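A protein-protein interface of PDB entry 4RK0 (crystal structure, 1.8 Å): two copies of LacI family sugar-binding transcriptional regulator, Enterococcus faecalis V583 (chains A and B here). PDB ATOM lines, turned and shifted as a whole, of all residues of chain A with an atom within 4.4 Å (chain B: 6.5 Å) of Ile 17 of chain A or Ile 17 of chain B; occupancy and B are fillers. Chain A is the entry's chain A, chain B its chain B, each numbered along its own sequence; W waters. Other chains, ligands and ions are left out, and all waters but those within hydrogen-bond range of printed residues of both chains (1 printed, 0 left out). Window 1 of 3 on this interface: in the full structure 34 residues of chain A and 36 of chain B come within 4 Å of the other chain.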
ATOM      1  N   VAL A  14      -3.547  -7.319  12.056  1.00  0.00           N
ATOM      2  CA  VAL A  14      -3.772  -8.726  11.728  1.00  0.00           C
ATOM      3  C   VAL A  14      -3.244  -9.018  10.315  1.00  0.00           C
ATOM      4  O   VAL A  14      -3.058  -8.091   9.542  1.00  0.00           O
ATOM      5  CB  VAL A  14      -5.268  -9.078  11.792  1.00  0.00           C
ATOM      6  CG1 VAL A  14      -5.763  -8.917  13.217  1.00  0.00           C
ATOM      7  CG2 VAL A  14      -6.051  -8.193  10.866  1.00  0.00           C
ATOM      8  N   ASP A  16      -4.762 -10.475   7.750  1.00  0.00           N
ATOM      9  CA  ASP A  16      -5.755 -10.141   6.745  1.00  0.00           C
ATOM     10  C   ASP A  16      -7.138 -10.061   7.387  1.00  0.00           C
ATOM     11  O   ASP A  16      -7.308 -10.432   8.541  1.00  0.00           O
ATOM     12  CB  ASP A  16      -5.739 -11.137   5.593  1.00  0.00           C
ATOM     13  CG  ASP A  16      -6.330 -12.470   5.971  1.00  0.00           C
ATOM     14  OD1 ASP A  16      -7.493 -12.501   6.445  1.00  0.00           O
ATOM     15  OD2 ASP A  16      -5.632 -13.480   5.822  1.00  0.00           O
ATOM     16  N   ILE A  17      -8.124  -9.580   6.641  1.00  0.00           N
ATOM     17  CA  ILE A  17      -9.499  -9.563   7.132  1.00  0.00           C
ATOM     18  C   ILE A  17     -10.444 -10.393   6.265  1.00  0.00           C
ATOM     19  O   ILE A  17     -11.632 -10.497   6.549  1.00  0.00           O
ATOM     20  CB  ILE A  17     -10.043  -8.127   7.246  1.00  0.00           C
ATOM     21  CG1 ILE A  17      -9.853  -7.336   5.941  1.00  0.00           C
ATOM     22  CG2 ILE A  17      -9.341  -7.427   8.399  1.00  0.00           C
ATOM     23  CD1 ILE A  17     -10.762  -6.131   5.824  1.00  0.00           C
ATOM     24  N   THR A  18      -9.911 -10.991   5.227  1.00  0.00           N
ATOM     25  CA  THR A  18     -10.729 -11.795   4.331  1.00  0.00           C
ATOM     26  C   THR A  18     -10.883 -13.214   4.848  1.00  0.00           C
ATOM     27  O   THR A  18     -11.849 -13.892   4.501  1.00  0.00           O
ATOM     28  CB  THR A  18     -10.120 -11.870   2.939  1.00  0.00           C
ATOM     29  OG1 THR A  18      -8.754 -12.256   3.046  1.00  0.00           O
ATOM     30  CG2 THR A  18     -10.202 -10.531   2.256  1.00  0.00           C
ATOM     31  N   ASN A  19      -9.937 -13.665   5.677  1.00  0.00           N
ATOM     32  CA  ASN A  19     -10.039 -14.976   6.275  1.00  0.00           C
ATOM     33  C   ASN A  19     -11.095 -14.826   7.374  1.00  0.00           C
ATOM     34  O   ASN A  19     -10.943 -13.989   8.277  1.00  0.00           O
ATOM     35  CB  ASN A  19      -8.704 -15.372   6.868  1.00  0.00           C
ATOM     36  CG  ASN A  19      -8.736 -16.696   7.577  1.00  0.00           C
ATOM     37  OD1 ASN A  19      -9.778 -17.247   7.911  1.00  0.00           O
ATOM     38  ND2 ASN A  19      -7.559 -17.207   7.836  1.00  0.00           N
ATOM     39  N   ALA A  23     -11.652 -12.084  10.732  1.00  0.00           N
ATOM     40  CA  ALA A  23     -12.845 -11.241  10.848  1.00  0.00           C
ATOM     41  C   ALA A  23     -13.563 -11.471  12.174  1.00  0.00           C
ATOM     42  O   ALA A  23     -14.025 -10.513  12.806  1.00  0.00           O
ATOM     43  CB  ALA A  23     -13.790 -11.460   9.663  1.00  0.00           C
ATOM     44  N   ILE A  26     -11.665  -9.913  15.031  1.00  0.00           N
ATOM     45  CA  ILE A  26     -11.975  -8.503  15.115  1.00  0.00           C
ATOM     46  C   ILE A  26     -13.340  -8.258  15.811  1.00  0.00           C
ATOM     47  O   ILE A  26     -13.425  -7.425  16.691  1.00  0.00           O
ATOM     48  CB  ILE A  26     -11.877  -7.801  13.744  1.00  0.00           C
ATOM     49  CG1 ILE A  26     -10.396  -7.661  13.331  1.00  0.00           C
ATOM     50  CG2 ILE A  26     -12.540  -6.437  13.770  1.00  0.00           C
ATOM     51  CD1 ILE A  26     -10.205  -7.612  11.839  1.00  0.00           C
ATOM     52  N   LEU A  42      -7.712  -0.140  12.304  1.00  0.00           N
ATOM     53  CA  LEU A  42      -7.525  -1.417  11.656  1.00  0.00           C
ATOM     54  C   LEU A  42      -6.339  -1.378  10.719  1.00  0.00           C
ATOM     55  O   LEU A  42      -6.274  -0.541   9.821  1.00  0.00           O
ATOM     56  CB  LEU A  42      -8.770  -1.808  10.873  1.00  0.00           C
ATOM     57  CG  LEU A  42      -8.618  -3.153  10.164  1.00  0.00           C
ATOM     58  CD1 LEU A  42      -8.616  -4.307  11.137  1.00  0.00           C
ATOM     59  CD2 LEU A  42      -9.732  -3.282   9.147  1.00  0.00           C
ATOM     60  N   ASN A  44      -4.629  -4.328   8.465  1.00  0.00           N
ATOM     61  CA  ASN A  44      -4.376  -5.672   7.991  1.00  0.00           C
ATOM     62  C   ASN A  44      -3.185  -5.632   7.063  1.00  0.00           C
ATOM     63  O   ASN A  44      -3.124  -4.841   6.109  1.00  0.00           O
ATOM     64  CB  ASN A  44      -5.601  -6.318   7.331  1.00  0.00           C
ATOM     65  CG  ASN A  44      -6.341  -5.374   6.441  1.00  0.00           C
ATOM     66  OD1 ASN A  44      -6.898  -4.382   6.917  1.00  0.00           O
ATOM     67  ND2 ASN A  44      -6.369  -5.671   5.143  1.00  0.00           N
ATOM     68  N   VAL B  14     -19.344   0.123   8.376  1.00  0.00           N
ATOM     69  CA  VAL B  14     -19.927  -0.959   7.577  1.00  0.00           C
ATOM     70  C   VAL B  14     -20.846  -1.793   8.445  1.00  0.00           C
ATOM     71  O   VAL B  14     -20.694  -1.818   9.674  1.00  0.00           O
ATOM     72  CB  VAL B  14     -18.881  -1.915   6.973  1.00  0.00           C
ATOM     73  CG1 VAL B  14     -17.976  -1.192   6.009  1.00  0.00           C
ATOM     74  CG2 VAL B  14     -18.087  -2.617   8.042  1.00  0.00           C
ATOM     75  N   PRO B  15     -21.807  -2.489   7.811  1.00  0.00           N
ATOM     76  CA  PRO B  15     -22.710  -3.343   8.566  1.00  0.00           C
ATOM     77  C   PRO B  15     -21.960  -4.430   9.359  1.00  0.00           C
ATOM     78  O   PRO B  15     -22.095  -4.488  10.587  1.00  0.00           O
ATOM     79  CB  PRO B  15     -23.676  -3.884   7.475  1.00  0.00           C
ATOM     80  CG  PRO B  15     -23.693  -2.784   6.462  1.00  0.00           C
ATOM     81  CD  PRO B  15     -22.267  -2.313   6.417  1.00  0.00           C
ATOM     82  N   ASP B  16     -21.146  -5.239   8.693  1.00  0.00           N
ATOM     83  CA  ASP B  16     -20.272  -6.165   9.378  1.00  0.00           C
ATOM     84  C   ASP B  16     -19.189  -6.737   8.474  1.00  0.00           C
ATOM     85  O   ASP B  16     -19.453  -7.223   7.376  1.00  0.00           O
ATOM     86  CB  ASP B  16     -21.040  -7.328  10.017  1.00  0.00           C
ATOM     87  CG  ASP B  16     -20.237  -8.009  11.129  1.00  0.00           C
ATOM     88  OD1 ASP B  16     -19.308  -8.770  10.791  1.00  0.00           O
ATOM     89  OD2 ASP B  16     -20.510  -7.771  12.333  1.00  0.00           O
ATOM     90  N   ILE B  17     -17.979  -6.728   9.014  1.00  0.00           N
ATOM     91  CA  ILE B  17     -16.756  -7.198   8.365  1.00  0.00           C
ATOM     92  C   ILE B  17     -16.689  -8.728   8.159  1.00  0.00           C
ATOM     93  O   ILE B  17     -15.878  -9.214   7.374  1.00  0.00           O
ATOM     94  CB  ILE B  17     -15.537  -6.781   9.247  1.00  0.00           C
ATOM     95  CG1 ILE B  17     -14.206  -6.976   8.511  1.00  0.00           C
ATOM     96  CG2 ILE B  17     -15.518  -7.560  10.561  1.00  0.00           C
ATOM     97  CD1 ILE B  17     -13.005  -6.514   9.302  1.00  0.00           C
ATOM     98  N   THR B  18     -17.532  -9.483   8.850  1.00  0.00           N
ATOM     99  CA  THR B  18     -17.587 -10.922   8.635  1.00  0.00           C
ATOM    100  C   THR B  18     -18.277 -11.300   7.340  1.00  0.00           C
ATOM    101  O   THR B  18     -18.207 -12.441   6.935  1.00  0.00           O
ATOM    102  CB  THR B  18     -18.331 -11.639   9.760  1.00  0.00           C
ATOM    103  OG1 THR B  18     -19.568 -10.961  10.014  1.00  0.00           O
ATOM    104  CG2 THR B  18     -17.466 -11.648  11.000  1.00  0.00           C
ATOM    105  N   ASN B  19     -18.922 -10.359   6.679  1.00  0.00           N
ATOM    106  CA  ASN B  19     -19.397 -10.630   5.335  1.00  0.00           C
ATOM    107  C   ASN B  19     -18.289 -10.323   4.374  1.00  0.00           C
ATOM    108  O   ASN B  19     -17.848  -9.172   4.287  1.00  0.00           O
ATOM    109  CB  ASN B  19     -20.606  -9.790   5.031  1.00  0.00           C
ATOM    110  CG  ASN B  19     -21.166 -10.042   3.662  1.00  0.00           C
ATOM    111  OD1 ASN B  19     -20.546 -10.651   2.765  1.00  0.00           O
ATOM    112  ND2 ASN B  19     -22.356  -9.560   3.481  1.00  0.00           N
ATOM    113  N   PRO B  20     -17.839 -11.337   3.619  1.00  0.00           N
ATOM    114  CA  PRO B  20     -16.699 -11.150   2.743  1.00  0.00           C
ATOM    115  C   PRO B  20     -16.861  -9.951   1.850  1.00  0.00           C
ATOM    116  O   PRO B  20     -15.869  -9.306   1.553  1.00  0.00           O
ATOM    117  CB  PRO B  20     -16.652 -12.460   1.912  1.00  0.00           C
ATOM    118  CG  PRO B  20     -17.365 -13.453   2.726  1.00  0.00           C
ATOM    119  CD  PRO B  20     -18.384 -12.714   3.533  1.00  0.00           C
ATOM    120  N   PHE B  21     -18.096  -9.642   1.418  1.00  0.00           N
ATOM    121  CA  PHE B  21     -18.319  -8.421   0.654  1.00  0.00           C
ATOM    122  C   PHE B  21     -17.692  -7.171   1.360  1.00  0.00           C
ATOM    123  O   PHE B  21     -16.903  -6.426   0.761  1.00  0.00           O
ATOM    124  CB  PHE B  21     -19.794  -8.212   0.429  1.00  0.00           C
ATOM    125  CG  PHE B  21     -20.117  -6.949  -0.314  1.00  0.00           C
ATOM    126  CD1 PHE B  21     -20.026  -6.897  -1.703  1.00  0.00           C
ATOM    127  CD2 PHE B  21     -20.474  -5.815   0.374  1.00  0.00           C
ATOM    128  CE1 PHE B  21     -20.329  -5.721  -2.387  1.00  0.00           C
ATOM    129  CE2 PHE B  21     -20.771  -4.634  -0.303  1.00  0.00           C
ATOM    130  CZ  PHE B  21     -20.707  -4.593  -1.682  1.00  0.00           C
ATOM    131  N   PHE B  22     -18.019  -6.983   2.628  1.00  0.00           N
ATOM    132  CA  PHE B  22     -17.528  -5.842   3.355  1.00  0.00           C
ATOM    133  C   PHE B  22     -16.031  -5.909   3.651  1.00  0.00           C
ATOM    134  O   PHE B  22     -15.364  -4.855   3.652  1.00  0.00           O
ATOM    135  CB  PHE B  22     -18.399  -5.532   4.582  1.00  0.00           C
ATOM    136  CG  PHE B  22     -19.809  -5.108   4.218  1.00  0.00           C
ATOM    137  CD1 PHE B  22     -20.027  -3.913   3.533  1.00  0.00           C
ATOM    138  CD2 PHE B  22     -20.894  -5.911   4.505  1.00  0.00           C
ATOM    139  CE1 PHE B  22     -21.297  -3.517   3.171  1.00  0.00           C
ATOM    140  CE2 PHE B  22     -22.184  -5.530   4.137  1.00  0.00           C
ATOM    141  CZ  PHE B  22     -22.377  -4.324   3.467  1.00  0.00           C
ATOM    142  N   ALA B  23     -15.504  -7.102   3.873  1.00  0.00           N
ATOM    143  CA  ALA B  23     -14.044  -7.293   3.963  1.00  0.00           C
ATOM    144  C   ALA B  23     -13.345  -6.780   2.704  1.00  0.00           C
ATOM    145  O   ALA B  23     -12.344  -6.063   2.787  1.00  0.00           O
ATOM    146  CB  ALA B  23     -13.709  -8.756   4.223  1.00  0.00           C
ATOM    147  N   GLN B  24     -13.874  -7.141   1.529  1.00  0.00           N
ATOM    148  CA  GLN B  24     -13.249  -6.738   0.277  1.00  0.00           C
ATOM    149  C   GLN B  24     -13.447  -5.237   0.021  1.00  0.00           C
ATOM    150  O   GLN B  24     -12.590  -4.575  -0.529  1.00  0.00           O
ATOM    151  CB  GLN B  24     -13.801  -7.575  -0.870  1.00  0.00           C
ATOM    152  CG  GLN B  24     -13.335  -9.017  -0.822  1.00  0.00           C
ATOM    153  CD  GLN B  24     -11.842  -9.188  -1.082  1.00  0.00           C
ATOM    154  OE1 GLN B  24     -11.199  -8.340  -1.689  1.00  0.00           O
ATOM    155  NE2 GLN B  24     -11.295 -10.302  -0.635  1.00  0.00           N
ATOM    156  N   ILE B  26     -13.385  -2.981   2.313  1.00  0.00           N
ATOM    157  CA  ILE B  26     -12.406  -2.345   3.178  1.00  0.00           C
ATOM    158  C   ILE B  26     -11.042  -2.432   2.531  1.00  0.00           C
ATOM    159  O   ILE B  26     -10.292  -1.465   2.527  1.00  0.00           O
ATOM    160  CB  ILE B  26     -12.421  -2.991   4.572  1.00  0.00           C
ATOM    161  CG1 ILE B  26     -13.670  -2.487   5.324  1.00  0.00           C
ATOM    162  CG2 ILE B  26     -11.130  -2.721   5.337  1.00  0.00           C
ATOM    163  CD1 ILE B  26     -13.930  -3.235   6.596  1.00  0.00           C
ATOM    164  N   ARG B  27     -10.752  -3.584   1.943  1.00  0.00           N
ATOM    165  CA  ARG B  27      -9.519  -3.750   1.187  1.00  0.00           C
ATOM    166  C   ARG B  27      -9.363  -2.743   0.069  1.00  0.00           C
ATOM    167  O   ARG B  27      -8.269  -2.182  -0.100  1.00  0.00           O
ATOM    168  CB  ARG B  27      -9.392  -5.155   0.637  1.00  0.00           C
ATOM    169  CG  ARG B  27      -9.033  -6.143   1.709  1.00  0.00           C
ATOM    170  CD  ARG B  27      -8.834  -7.541   1.153  1.00  0.00           C
ATOM    171  NE  ARG B  27      -7.542  -7.707   0.493  1.00  0.00           N
ATOM    172  CZ  ARG B  27      -7.336  -7.717  -0.824  1.00  0.00           C
ATOM    173  NH1 ARG B  27      -6.100  -7.871  -1.279  1.00  0.00           N
ATOM    174  NH2 ARG B  27      -8.335  -7.575  -1.703  1.00  0.00           N
ATOM    175  N   GLU B  30      -8.605   0.658   1.724  1.00  0.00           N
ATOM    176  CA  GLU B  30      -7.259   0.619   2.208  1.00  0.00           C
ATOM    177  C   GLU B  30      -6.193   0.751   1.132  1.00  0.00           C
ATOM    178  O   GLU B  30      -5.092   1.242   1.407  1.00  0.00           O
ATOM    179  CB  GLU B  30      -7.002  -0.682   2.942  1.00  0.00           C
ATOM    180  CG  GLU B  30      -7.694  -0.795   4.300  1.00  0.00           C
ATOM    181  CD  GLU B  30      -7.629  -2.194   4.873  1.00  0.00           C
ATOM    182  OE1 GLU B  30      -7.360  -3.170   4.112  1.00  0.00           O
ATOM    183  OE2 GLU B  30      -7.823  -2.325   6.101  1.00  0.00           O
ATOM    184  N   LEU B  42     -12.335   1.495  12.182  1.00  0.00           N
ATOM    185  CA  LEU B  42     -13.380   0.614  11.731  1.00  0.00           C
ATOM    186  C   LEU B  42     -14.534   0.714  12.712  1.00  0.00           C
ATOM    187  O   LEU B  42     -14.324   0.743  13.914  1.00  0.00           O
ATOM    188  CB  LEU B  42     -12.838  -0.813  11.708  1.00  0.00           C
ATOM    189  CG  LEU B  42     -13.886  -1.887  11.418  1.00  0.00           C
ATOM    190  CD1 LEU B  42     -14.283  -1.787   9.964  1.00  0.00           C
ATOM    191  CD2 LEU B  42     -13.348  -3.272  11.775  1.00  0.00           C
ATOM    192  N   ASN B  44     -18.001  -1.663  12.966  1.00  0.00           N
ATOM    193  CA  ASN B  44     -19.018  -2.617  12.516  1.00  0.00           C
ATOM    194  C   ASN B  44     -20.334  -2.224  13.115  1.00  0.00           C
ATOM    195  O   ASN B  44     -20.611  -2.505  14.283  1.00  0.00           O
ATOM    196  CB  ASN B  44     -18.731  -4.027  12.994  1.00  0.00           C
ATOM    197  CG  ASN B  44     -17.629  -4.678  12.243  1.00  0.00           C
ATOM    198  OD1 ASN B  44     -17.547  -4.568  11.023  1.00  0.00           O
ATOM    199  ND2 ASN B  44     -16.769  -5.378  12.962  1.00  0.00           N
ATOM    200  N   GLN B  47     -22.510  -4.450  15.456  1.00  0.00           N
ATOM    201  CA  GLN B  47     -22.205  -4.810  16.828  1.00  0.00           C
ATOM    202  C   GLN B  47     -22.612  -3.777  17.879  1.00  0.00           C
ATOM    203  O   GLN B  47     -22.371  -4.004  19.061  1.00  0.00           O
ATOM    204  CB  GLN B  47     -20.731  -5.140  16.968  1.00  0.00           C
ATOM    205  CG  GLN B  47     -20.337  -6.353  16.164  1.00  0.00           C
ATOM    206  CD  GLN B  47     -18.925  -6.734  16.467  1.00  0.00           C
ATOM    207  OE1 GLN B  47     -18.000  -6.281  15.789  1.00  0.00           O
ATOM    208  NE2 GLN B  47     -18.733  -7.519  17.523  1.00  0.00           N
HETATM  209  O   HOH W   1     -14.368 -11.313   6.119  1.00  0.00           O
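Ile 17 of chain B touches its own counterpart, Ile 17 of chain A.
Ile 17 of chain A touches Ala 23 of chain B, and with the chains exchanged Ala 23 of chain A touches Ile 17 of chain B.
Ile 17 of chain A touches Ile 26 of chain B, and with the chains exchanged Ile 26 of chain A touches Ile 17 of chain B.
Ile 26 of chain A touches Leu 42 of chain B, but with the chains exchanged Leu 42 of chain A does not touch Ile 26 of chain B (4.1 Å).
Of chain B, only Ile 17 (3.9 Å), Ala 23 (3.4 Å) and Ile 26 (3.5 Å) come within 4 Å of Ile 17 of chain A.
Of chain A, only Ile 17, Ala 23 and Ile 26 come within 4 Å of Ile 17 of chain B.
Of the printed residues of chain A, Thr 18 of chain B touches Ala 23.
Of the printed residues of chain A, Glu 30 of chain B touches Leu 42 and Asn 44.
Of the printed residues of chain A, Gln 24 of chain B touches Thr 18.
Phe 21 of chain B touches none of the printed residues of chain A.
The nearest printed residue of chain B that does not touch Leu 42 of chain A is Ile 26 of chain B (4.1 Å).
Ile 17 of chain A touches Ile 17 of chain B.
Ile 17 of chain A touches Ala 23 of chain B.
Ile 26 of chain B touches Ile 17 of chain A (CG2 to CD1, 3.5 Å).
Thr 18 of chain A touches Gln 24 of chain B (CG2 to NE2, 3.1 Å).
Arg 27 of chain B touches Thr 18 of chain A.
Ala 23 of chain A touches Ile 17 of chain B (CB to O, 3.8 Å).
CB of Ala 23 of chain A touches CG2 of Thr 18 of chain B, 3.9 Å away.
Ile 26 of chain A touches Ile 17 of chain B.
Ile 26 of chain A touches Leu 42 of chain B (CG2 to CD2, 3.8 Å).
OE2 of Glu 30 of chain B touches CD2 of Leu 42 of chain A (3.7 Å).
N of Thr 18 of chain A is in hydrogen-bond range of OD1 of Asp 16 of chain A (3.1 Å).
OD1 of Asp 16 of chain B sits at hydrogen-bond distance from N of Thr 18 of chain B (2.7 Å).
The backbone NH (N) of Ile 17 of chain B sits at hydrogen-bond distance from the side-chain amide oxygen (OD1) of Asn 44 of chain B.
The side-chain amide oxygen (OE1) of Gln 24 of chain B sits at hydrogen-bond distance from the guanidinium group (NH2) of Arg 27 of chain B (3.0 Å).
Hydrophobic or aromatic side chains of chain A that line the printed part of chain B: Ile 17, Ala 23, Ile 26 and Leu 42.
Among the printed residues, 11 pairs touch across the chains.
Among the printed residues, no Asp or Glu carboxylate lies within 4 Å of a Lys or Arg side-chain nitrogen of the other chain.
OE1 of Glu 30 of chain B sits at hydrogen-bond distance from ND2 of Asn 44 of chain A, at 2.9 Å.
Water W1 lies within hydrogen-bond range of O of Ile 17 of chain B (2.9 Å) and O of Ile 17 of chain A (2.9 Å).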
